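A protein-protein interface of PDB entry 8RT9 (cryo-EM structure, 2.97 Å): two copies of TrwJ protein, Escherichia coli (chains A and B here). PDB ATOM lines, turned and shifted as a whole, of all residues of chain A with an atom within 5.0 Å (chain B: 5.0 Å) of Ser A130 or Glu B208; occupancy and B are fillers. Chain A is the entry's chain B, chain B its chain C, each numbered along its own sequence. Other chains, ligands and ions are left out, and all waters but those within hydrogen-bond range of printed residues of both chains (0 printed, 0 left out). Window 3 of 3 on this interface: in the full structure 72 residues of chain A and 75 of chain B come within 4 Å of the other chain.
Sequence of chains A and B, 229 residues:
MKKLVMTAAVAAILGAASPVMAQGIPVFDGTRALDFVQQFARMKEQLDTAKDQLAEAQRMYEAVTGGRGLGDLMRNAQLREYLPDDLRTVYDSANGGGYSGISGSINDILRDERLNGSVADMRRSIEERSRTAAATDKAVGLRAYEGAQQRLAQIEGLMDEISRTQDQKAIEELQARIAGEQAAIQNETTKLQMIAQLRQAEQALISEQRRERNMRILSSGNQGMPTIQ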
ATOM      1  N   ILE A 126     -20.343 -17.117 -25.049  1.00  0.00           N
ATOM      2  CA  ILE A 126     -19.042 -17.394 -24.452  1.00  0.00           C
ATOM      3  C   ILE A 126     -18.388 -18.602 -25.112  1.00  0.00           C
ATOM      4  O   ILE A 126     -17.187 -18.583 -25.419  1.00  0.00           O
ATOM      5  CB  ILE A 126     -19.183 -17.573 -22.934  1.00  0.00           C
ATOM      6  CG1 ILE A 126     -19.539 -16.243 -22.282  1.00  0.00           C
ATOM      7  CG2 ILE A 126     -17.901 -18.108 -22.346  1.00  0.00           C
ATOM      8  CD1 ILE A 126     -20.088 -16.380 -20.900  1.00  0.00           C
ATOM      9  N   GLU A 127     -19.155 -19.669 -25.348  1.00  0.00           N
ATOM     10  CA  GLU A 127     -18.583 -20.840 -26.010  1.00  0.00           C
ATOM     11  C   GLU A 127     -18.122 -20.510 -27.422  1.00  0.00           C
ATOM     12  O   GLU A 127     -17.050 -20.961 -27.861  1.00  0.00           O
ATOM     13  CB  GLU A 127     -19.591 -21.984 -26.036  1.00  0.00           C
ATOM     14  CG  GLU A 127     -19.852 -22.595 -24.679  1.00  0.00           C
ATOM     15  CD  GLU A 127     -20.994 -23.583 -24.701  1.00  0.00           C
ATOM     16  OE1 GLU A 127     -21.189 -24.239 -25.746  1.00  0.00           O
ATOM     17  OE2 GLU A 127     -21.692 -23.714 -23.675  1.00  0.00           O
ATOM     18  N   GLU A 128     -18.917 -19.728 -28.153  1.00  0.00           N
ATOM     19  CA  GLU A 128     -18.503 -19.319 -29.485  1.00  0.00           C
ATOM     20  C   GLU A 128     -17.219 -18.505 -29.433  1.00  0.00           C
ATOM     21  O   GLU A 128     -16.322 -18.706 -30.258  1.00  0.00           O
ATOM     22  CB  GLU A 128     -19.617 -18.530 -30.167  1.00  0.00           C
ATOM     23  CG  GLU A 128     -20.665 -19.399 -30.825  1.00  0.00           C
ATOM     24  CD  GLU A 128     -21.675 -18.590 -31.614  1.00  0.00           C
ATOM     25  OE1 GLU A 128     -21.361 -17.440 -31.984  1.00  0.00           O
ATOM     26  OE2 GLU A 128     -22.781 -19.108 -31.870  1.00  0.00           O
ATOM     27  N   ARG A 129     -17.104 -17.588 -28.466  1.00  0.00           N
ATOM     28  CA  ARG A 129     -15.876 -16.812 -28.359  1.00  0.00           C
ATOM     29  C   ARG A 129     -14.680 -17.705 -28.094  1.00  0.00           C
ATOM     30  O   ARG A 129     -13.615 -17.508 -28.683  1.00  0.00           O
ATOM     31  CB  ARG A 129     -15.969 -15.756 -27.260  1.00  0.00           C
ATOM     32  CG  ARG A 129     -16.471 -14.423 -27.731  1.00  0.00           C
ATOM     33  CD  ARG A 129     -16.399 -13.394 -26.629  1.00  0.00           C
ATOM     34  NE  ARG A 129     -15.109 -12.715 -26.638  1.00  0.00           N
ATOM     35  CZ  ARG A 129     -14.718 -11.831 -25.730  1.00  0.00           C
ATOM     36  NH1 ARG A 129     -15.517 -11.508 -24.729  1.00  0.00           N
ATOM     37  NH2 ARG A 129     -13.527 -11.265 -25.828  1.00  0.00           N
ATOM     38  N   SER A 130     -14.830 -18.686 -27.209  1.00  0.00           N
ATOM     39  CA  SER A 130     -13.699 -19.551 -26.891  1.00  0.00           C
ATOM     40  C   SER A 130     -13.230 -20.320 -28.123  1.00  0.00           C
ATOM     41  O   SER A 130     -12.033 -20.318 -28.465  1.00  0.00           O
ATOM     42  CB  SER A 130     -14.085 -20.503 -25.765  1.00  0.00           C
ATOM     43  OG  SER A 130     -14.445 -19.787 -24.600  1.00  0.00           O
ATOM     44  N   ARG A 131     -14.167 -20.971 -28.813  1.00  0.00           N
ATOM     45  CA  ARG A 131     -13.794 -21.751 -29.988  1.00  0.00           C
ATOM     46  C   ARG A 131     -13.188 -20.866 -31.069  1.00  0.00           C
ATOM     47  O   ARG A 131     -12.154 -21.208 -31.664  1.00  0.00           O
ATOM     48  CB  ARG A 131     -15.013 -22.492 -30.528  1.00  0.00           C
ATOM     49  CG  ARG A 131     -15.599 -23.489 -29.565  1.00  0.00           C
ATOM     50  CD  ARG A 131     -16.769 -24.211 -30.189  1.00  0.00           C
ATOM     51  NE  ARG A 131     -16.517 -24.537 -31.586  1.00  0.00           N
ATOM     52  CZ  ARG A 131     -15.966 -25.673 -31.994  1.00  0.00           C
ATOM     53  NH1 ARG A 131     -15.609 -26.592 -31.111  1.00  0.00           N
ATOM     54  NH2 ARG A 131     -15.773 -25.891 -33.286  1.00  0.00           N
ATOM     55  N   THR A 132     -13.809 -19.715 -31.326  1.00  0.00           N
ATOM     56  CA  THR A 132     -13.314 -18.823 -32.360  1.00  0.00           C
ATOM     57  C   THR A 132     -11.942 -18.280 -32.006  1.00  0.00           C
ATOM     58  O   THR A 132     -11.105 -18.087 -32.888  1.00  0.00           O
ATOM     59  CB  THR A 132     -14.302 -17.682 -32.582  1.00  0.00           C
ATOM     60  OG1 THR A 132     -15.590 -18.223 -32.890  1.00  0.00           O
ATOM     61  CG2 THR A 132     -13.853 -16.802 -33.729  1.00  0.00           C
ATOM     62  N   ALA A 133     -11.686 -18.034 -30.723  1.00  0.00           N
ATOM     63  CA  ALA A 133     -10.382 -17.530 -30.318  1.00  0.00           C
ATOM     64  C   ALA A 133      -9.295 -18.558 -30.580  1.00  0.00           C
ATOM     65  O   ALA A 133      -8.228 -18.229 -31.116  1.00  0.00           O
ATOM     66  CB  ALA A 133     -10.412 -17.137 -28.843  1.00  0.00           C
ATOM     67  N   ALA A 134      -9.549 -19.815 -30.217  1.00  0.00           N
ATOM     68  CA  ALA A 134      -8.552 -20.848 -30.484  1.00  0.00           C
ATOM     69  C   ALA A 134      -8.287 -20.979 -31.981  1.00  0.00           C
ATOM     70  O   ALA A 134      -7.128 -21.018 -32.429  1.00  0.00           O
ATOM     71  CB  ALA A 134      -9.008 -22.180 -29.895  1.00  0.00           C
ATOM     72  N   ILE A 206     -12.478 -13.478 -21.993  1.00  0.00           N
ATOM     73  CA  ILE A 206     -13.417 -14.597 -21.997  1.00  0.00           C
ATOM     74  C   ILE A 206     -13.622 -15.116 -20.581  1.00  0.00           C
ATOM     75  O   ILE A 206     -14.749 -15.429 -20.173  1.00  0.00           O
ATOM     76  CB  ILE A 206     -12.932 -15.707 -22.943  1.00  0.00           C
ATOM     77  CG1 ILE A 206     -12.980 -15.234 -24.390  1.00  0.00           C
ATOM     78  CG2 ILE A 206     -13.782 -16.942 -22.794  1.00  0.00           C
ATOM     79  CD1 ILE A 206     -12.364 -16.209 -25.356  1.00  0.00           C
ATOM     80  N   ARG A 210     -17.120 -15.271 -18.417  1.00  0.00           N
ATOM     81  CA  ARG A 210     -17.577 -16.464 -17.716  1.00  0.00           C
ATOM     82  C   ARG A 210     -17.924 -16.136 -16.278  1.00  0.00           C
ATOM     83  O   ARG A 210     -18.963 -16.563 -15.759  1.00  0.00           O
ATOM     84  CB  ARG A 210     -16.505 -17.546 -17.732  1.00  0.00           C
ATOM     85  CG  ARG A 210     -16.311 -18.216 -19.050  1.00  0.00           C
ATOM     86  CD  ARG A 210     -15.321 -19.346 -18.931  1.00  0.00           C
ATOM     87  NE  ARG A 210     -14.802 -19.714 -20.236  1.00  0.00           N
ATOM     88  CZ  ARG A 210     -15.409 -20.565 -21.048  1.00  0.00           C
ATOM     89  NH1 ARG A 210     -16.577 -21.077 -20.693  1.00  0.00           N
ATOM     90  NH2 ARG A 210     -14.881 -20.864 -22.225  1.00  0.00           N
ATOM     91  N   ALA B 204      -5.060 -24.868 -26.528  1.00  0.00           N
ATOM     92  CA  ALA B 204      -6.425 -24.375 -26.394  1.00  0.00           C
ATOM     93  C   ALA B 204      -7.411 -25.273 -27.128  1.00  0.00           C
ATOM     94  O   ALA B 204      -8.507 -25.543 -26.627  1.00  0.00           O
ATOM     95  CB  ALA B 204      -6.521 -22.941 -26.911  1.00  0.00           C
ATOM     96  N   LEU B 205      -7.043 -25.742 -28.316  1.00  0.00           N
ATOM     97  CA  LEU B 205      -7.930 -26.615 -29.075  1.00  0.00           C
ATOM     98  C   LEU B 205      -8.141 -27.947 -28.370  1.00  0.00           C
ATOM     99  O   LEU B 205      -9.252 -28.493 -28.381  1.00  0.00           O
ATOM    100  CB  LEU B 205      -7.373 -26.832 -30.476  1.00  0.00           C
ATOM    101  CG  LEU B 205      -7.483 -25.643 -31.422  1.00  0.00           C
ATOM    102  CD1 LEU B 205      -6.683 -25.901 -32.672  1.00  0.00           C
ATOM    103  CD2 LEU B 205      -8.929 -25.387 -31.765  1.00  0.00           C
ATOM    104  N   ILE B 206      -7.088 -28.498 -27.769  1.00  0.00           N
ATOM    105  CA  ILE B 206      -7.245 -29.744 -27.021  1.00  0.00           C
ATOM    106  C   ILE B 206      -8.193 -29.538 -25.849  1.00  0.00           C
ATOM    107  O   ILE B 206      -9.048 -30.388 -25.562  1.00  0.00           O
ATOM    108  CB  ILE B 206      -5.877 -30.273 -26.558  1.00  0.00           C
ATOM    109  CG1 ILE B 206      -5.042 -30.712 -27.755  1.00  0.00           C
ATOM    110  CG2 ILE B 206      -6.050 -31.436 -25.617  1.00  0.00           C
ATOM    111  CD1 ILE B 206      -3.631 -31.086 -27.390  1.00  0.00           C
ATOM    112  N   SER B 207      -8.066 -28.406 -25.156  1.00  0.00           N
ATOM    113  CA  SER B 207      -8.993 -28.114 -24.068  1.00  0.00           C
ATOM    114  C   SER B 207     -10.424 -27.995 -24.580  1.00  0.00           C
ATOM    115  O   SER B 207     -11.371 -28.461 -23.932  1.00  0.00           O
ATOM    116  CB  SER B 207      -8.574 -26.836 -23.351  1.00  0.00           C
ATOM    117  OG  SER B 207      -9.444 -26.560 -22.270  1.00  0.00           O
ATOM    118  N   GLU B 208     -10.599 -27.369 -25.744  1.00  0.00           N
ATOM    119  CA  GLU B 208     -11.932 -27.235 -26.320  1.00  0.00           C
ATOM    120  C   GLU B 208     -12.531 -28.596 -26.636  1.00  0.00           C
ATOM    121  O   GLU B 208     -13.722 -28.824 -26.411  1.00  0.00           O
ATOM    122  CB  GLU B 208     -11.873 -26.381 -27.584  1.00  0.00           C
ATOM    123  CG  GLU B 208     -11.564 -24.916 -27.348  1.00  0.00           C
ATOM    124  CD  GLU B 208     -12.603 -24.187 -26.524  1.00  0.00           C
ATOM    125  OE1 GLU B 208     -13.638 -24.778 -26.156  1.00  0.00           O
ATOM    126  OE2 GLU B 208     -12.362 -23.003 -26.220  1.00  0.00           O
ATOM    127  N   GLN B 209     -11.723 -29.506 -27.175  1.00  0.00           N
ATOM    128  CA  GLN B 209     -12.211 -30.852 -27.457  1.00  0.00           C
ATOM    129  C   GLN B 209     -12.585 -31.585 -26.176  1.00  0.00           C
ATOM    130  O   GLN B 209     -13.597 -32.297 -26.131  1.00  0.00           O
ATOM    131  CB  GLN B 209     -11.164 -31.635 -28.240  1.00  0.00           C
ATOM    132  CG  GLN B 209     -11.149 -31.316 -29.712  1.00  0.00           C
ATOM    133  CD  GLN B 209     -10.386 -32.335 -30.509  1.00  0.00           C
ATOM    134  OE1 GLN B 209      -9.521 -33.024 -29.978  1.00  0.00           O
ATOM    135  NE2 GLN B 209     -10.698 -32.441 -31.790  1.00  0.00           N
ATOM    136  N   ARG B 210     -11.780 -31.421 -25.126  1.00  0.00           N
ATOM    137  CA  ARG B 210     -12.127 -32.023 -23.845  1.00  0.00           C
ATOM    138  C   ARG B 210     -13.481 -31.533 -23.374  1.00  0.00           C
ATOM    139  O   ARG B 210     -14.320 -32.319 -22.919  1.00  0.00           O
ATOM    140  CB  ARG B 210     -11.083 -31.685 -22.788  1.00  0.00           C
ATOM    141  CG  ARG B 210      -9.783 -32.399 -22.939  1.00  0.00           C
ATOM    142  CD  ARG B 210      -8.868 -32.089 -21.783  1.00  0.00           C
ATOM    143  NE  ARG B 210      -7.492 -32.407 -22.117  1.00  0.00           N
ATOM    144  CZ  ARG B 210      -6.969 -33.614 -21.978  1.00  0.00           C
ATOM    145  NH1 ARG B 210      -7.738 -34.611 -21.566  1.00  0.00           N
ATOM    146  NH2 ARG B 210      -5.702 -33.839 -22.297  1.00  0.00           N
ATOM    147  N   ARG B 211     -13.711 -30.229 -23.477  1.00  0.00           N
ATOM    148  CA  ARG B 211     -14.958 -29.676 -22.974  1.00  0.00           C
ATOM    149  C   ARG B 211     -16.134 -30.071 -23.851  1.00  0.00           C
ATOM    150  O   ARG B 211     -17.254 -30.238 -23.359  1.00  0.00           O
ATOM    151  CB  ARG B 211     -14.834 -28.167 -22.853  1.00  0.00           C
ATOM    152  CG  ARG B 211     -16.032 -27.518 -22.252  1.00  0.00           C
ATOM    153  CD  ARG B 211     -15.903 -26.039 -22.381  1.00  0.00           C
ATOM    154  NE  ARG B 211     -14.730 -25.613 -21.630  1.00  0.00           N
ATOM    155  CZ  ARG B 211     -14.634 -24.453 -21.001  1.00  0.00           C
ATOM    156  NH1 ARG B 211     -15.662 -23.628 -21.014  1.00  0.00           N
ATOM    157  NH2 ARG B 211     -13.532 -24.133 -20.340  1.00  0.00           N
ATOM    158  N   GLU B 212     -15.903 -30.240 -25.150  1.00  0.00           N
ATOM    159  CA  GLU B 212     -16.959 -30.756 -26.013  1.00  0.00           C
ATOM    160  C   GLU B 212     -17.359 -32.164 -25.604  1.00  0.00           C
ATOM    161  O   GLU B 212     -18.553 -32.484 -25.540  1.00  0.00           O
ATOM    162  CB  GLU B 212     -16.507 -30.735 -27.469  1.00  0.00           C
ATOM    163  CG  GLU B 212     -17.573 -31.192 -28.439  1.00  0.00           C
ATOM    164  CD  GLU B 212     -17.110 -31.143 -29.881  1.00  0.00           C
ATOM    165  OE1 GLU B 212     -15.904 -30.910 -30.115  1.00  0.00           O
ATOM    166  OE2 GLU B 212     -17.950 -31.343 -30.784  1.00  0.00           O
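The guanidinium group (NH1) of Arg B211 lies close to the guanidinium group (NH1) of Arg A210, at 2.7 Å.
OG of Ser A130 is in hydrogen-bond range of NH2 of Arg A210 (2.6 Å).
The side-chain hydroxyl (OG) of Ser A130 sits at hydrogen-bond distance from the backbone carbonyl oxygen (O) of Ile A126 (3.1 Å).
Among the printed residues, pairs that only touch across the chains: Ser A130 with Glu B208, Arg A131 with Glu B208, Ala A134 with Ala B204 and Ala A134 with Leu B205.
Ser A130 touches one residue of chain B.
Of chain A, only Ser A130 (3.1 Å) and Arg A131 (3.8 Å) come within 4 Å of Glu B208.
Of the printed residues of chain B, Ala A134 touches Ala B204 (3.96 Å) and Leu B205 (3.7 Å).
Printed residues of chain B within 4 Å of Arg A210: Arg B211.
Of the printed residues of chain B, Arg A131 touches Glu B208 (3.8 Å).
Printed residues of chain A within 4 Å of Leu B205: Ala A134 (3.7 Å).
Of the printed residues of chain A, Ala B204 touches Ala A134 (3.96 Å).
Ala A133 touches none of the printed residues of chain B.
Ile A206 touches none of the printed residues of chain B.
The nearest printed residue of chain B that does not touch Ser A130 is Arg B211 (5.4 Å).
The nearest residue of chain A that does not touch Glu B208 is Ala A134 (4.5 Å).
Among the printed residues, 5 pairs touch across the chains.
Positions printed for both chains: 206 and 210.
Of the 5 pairs that touch across the chains among the printed residues, none has its exchanged pair printed and touching as well.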
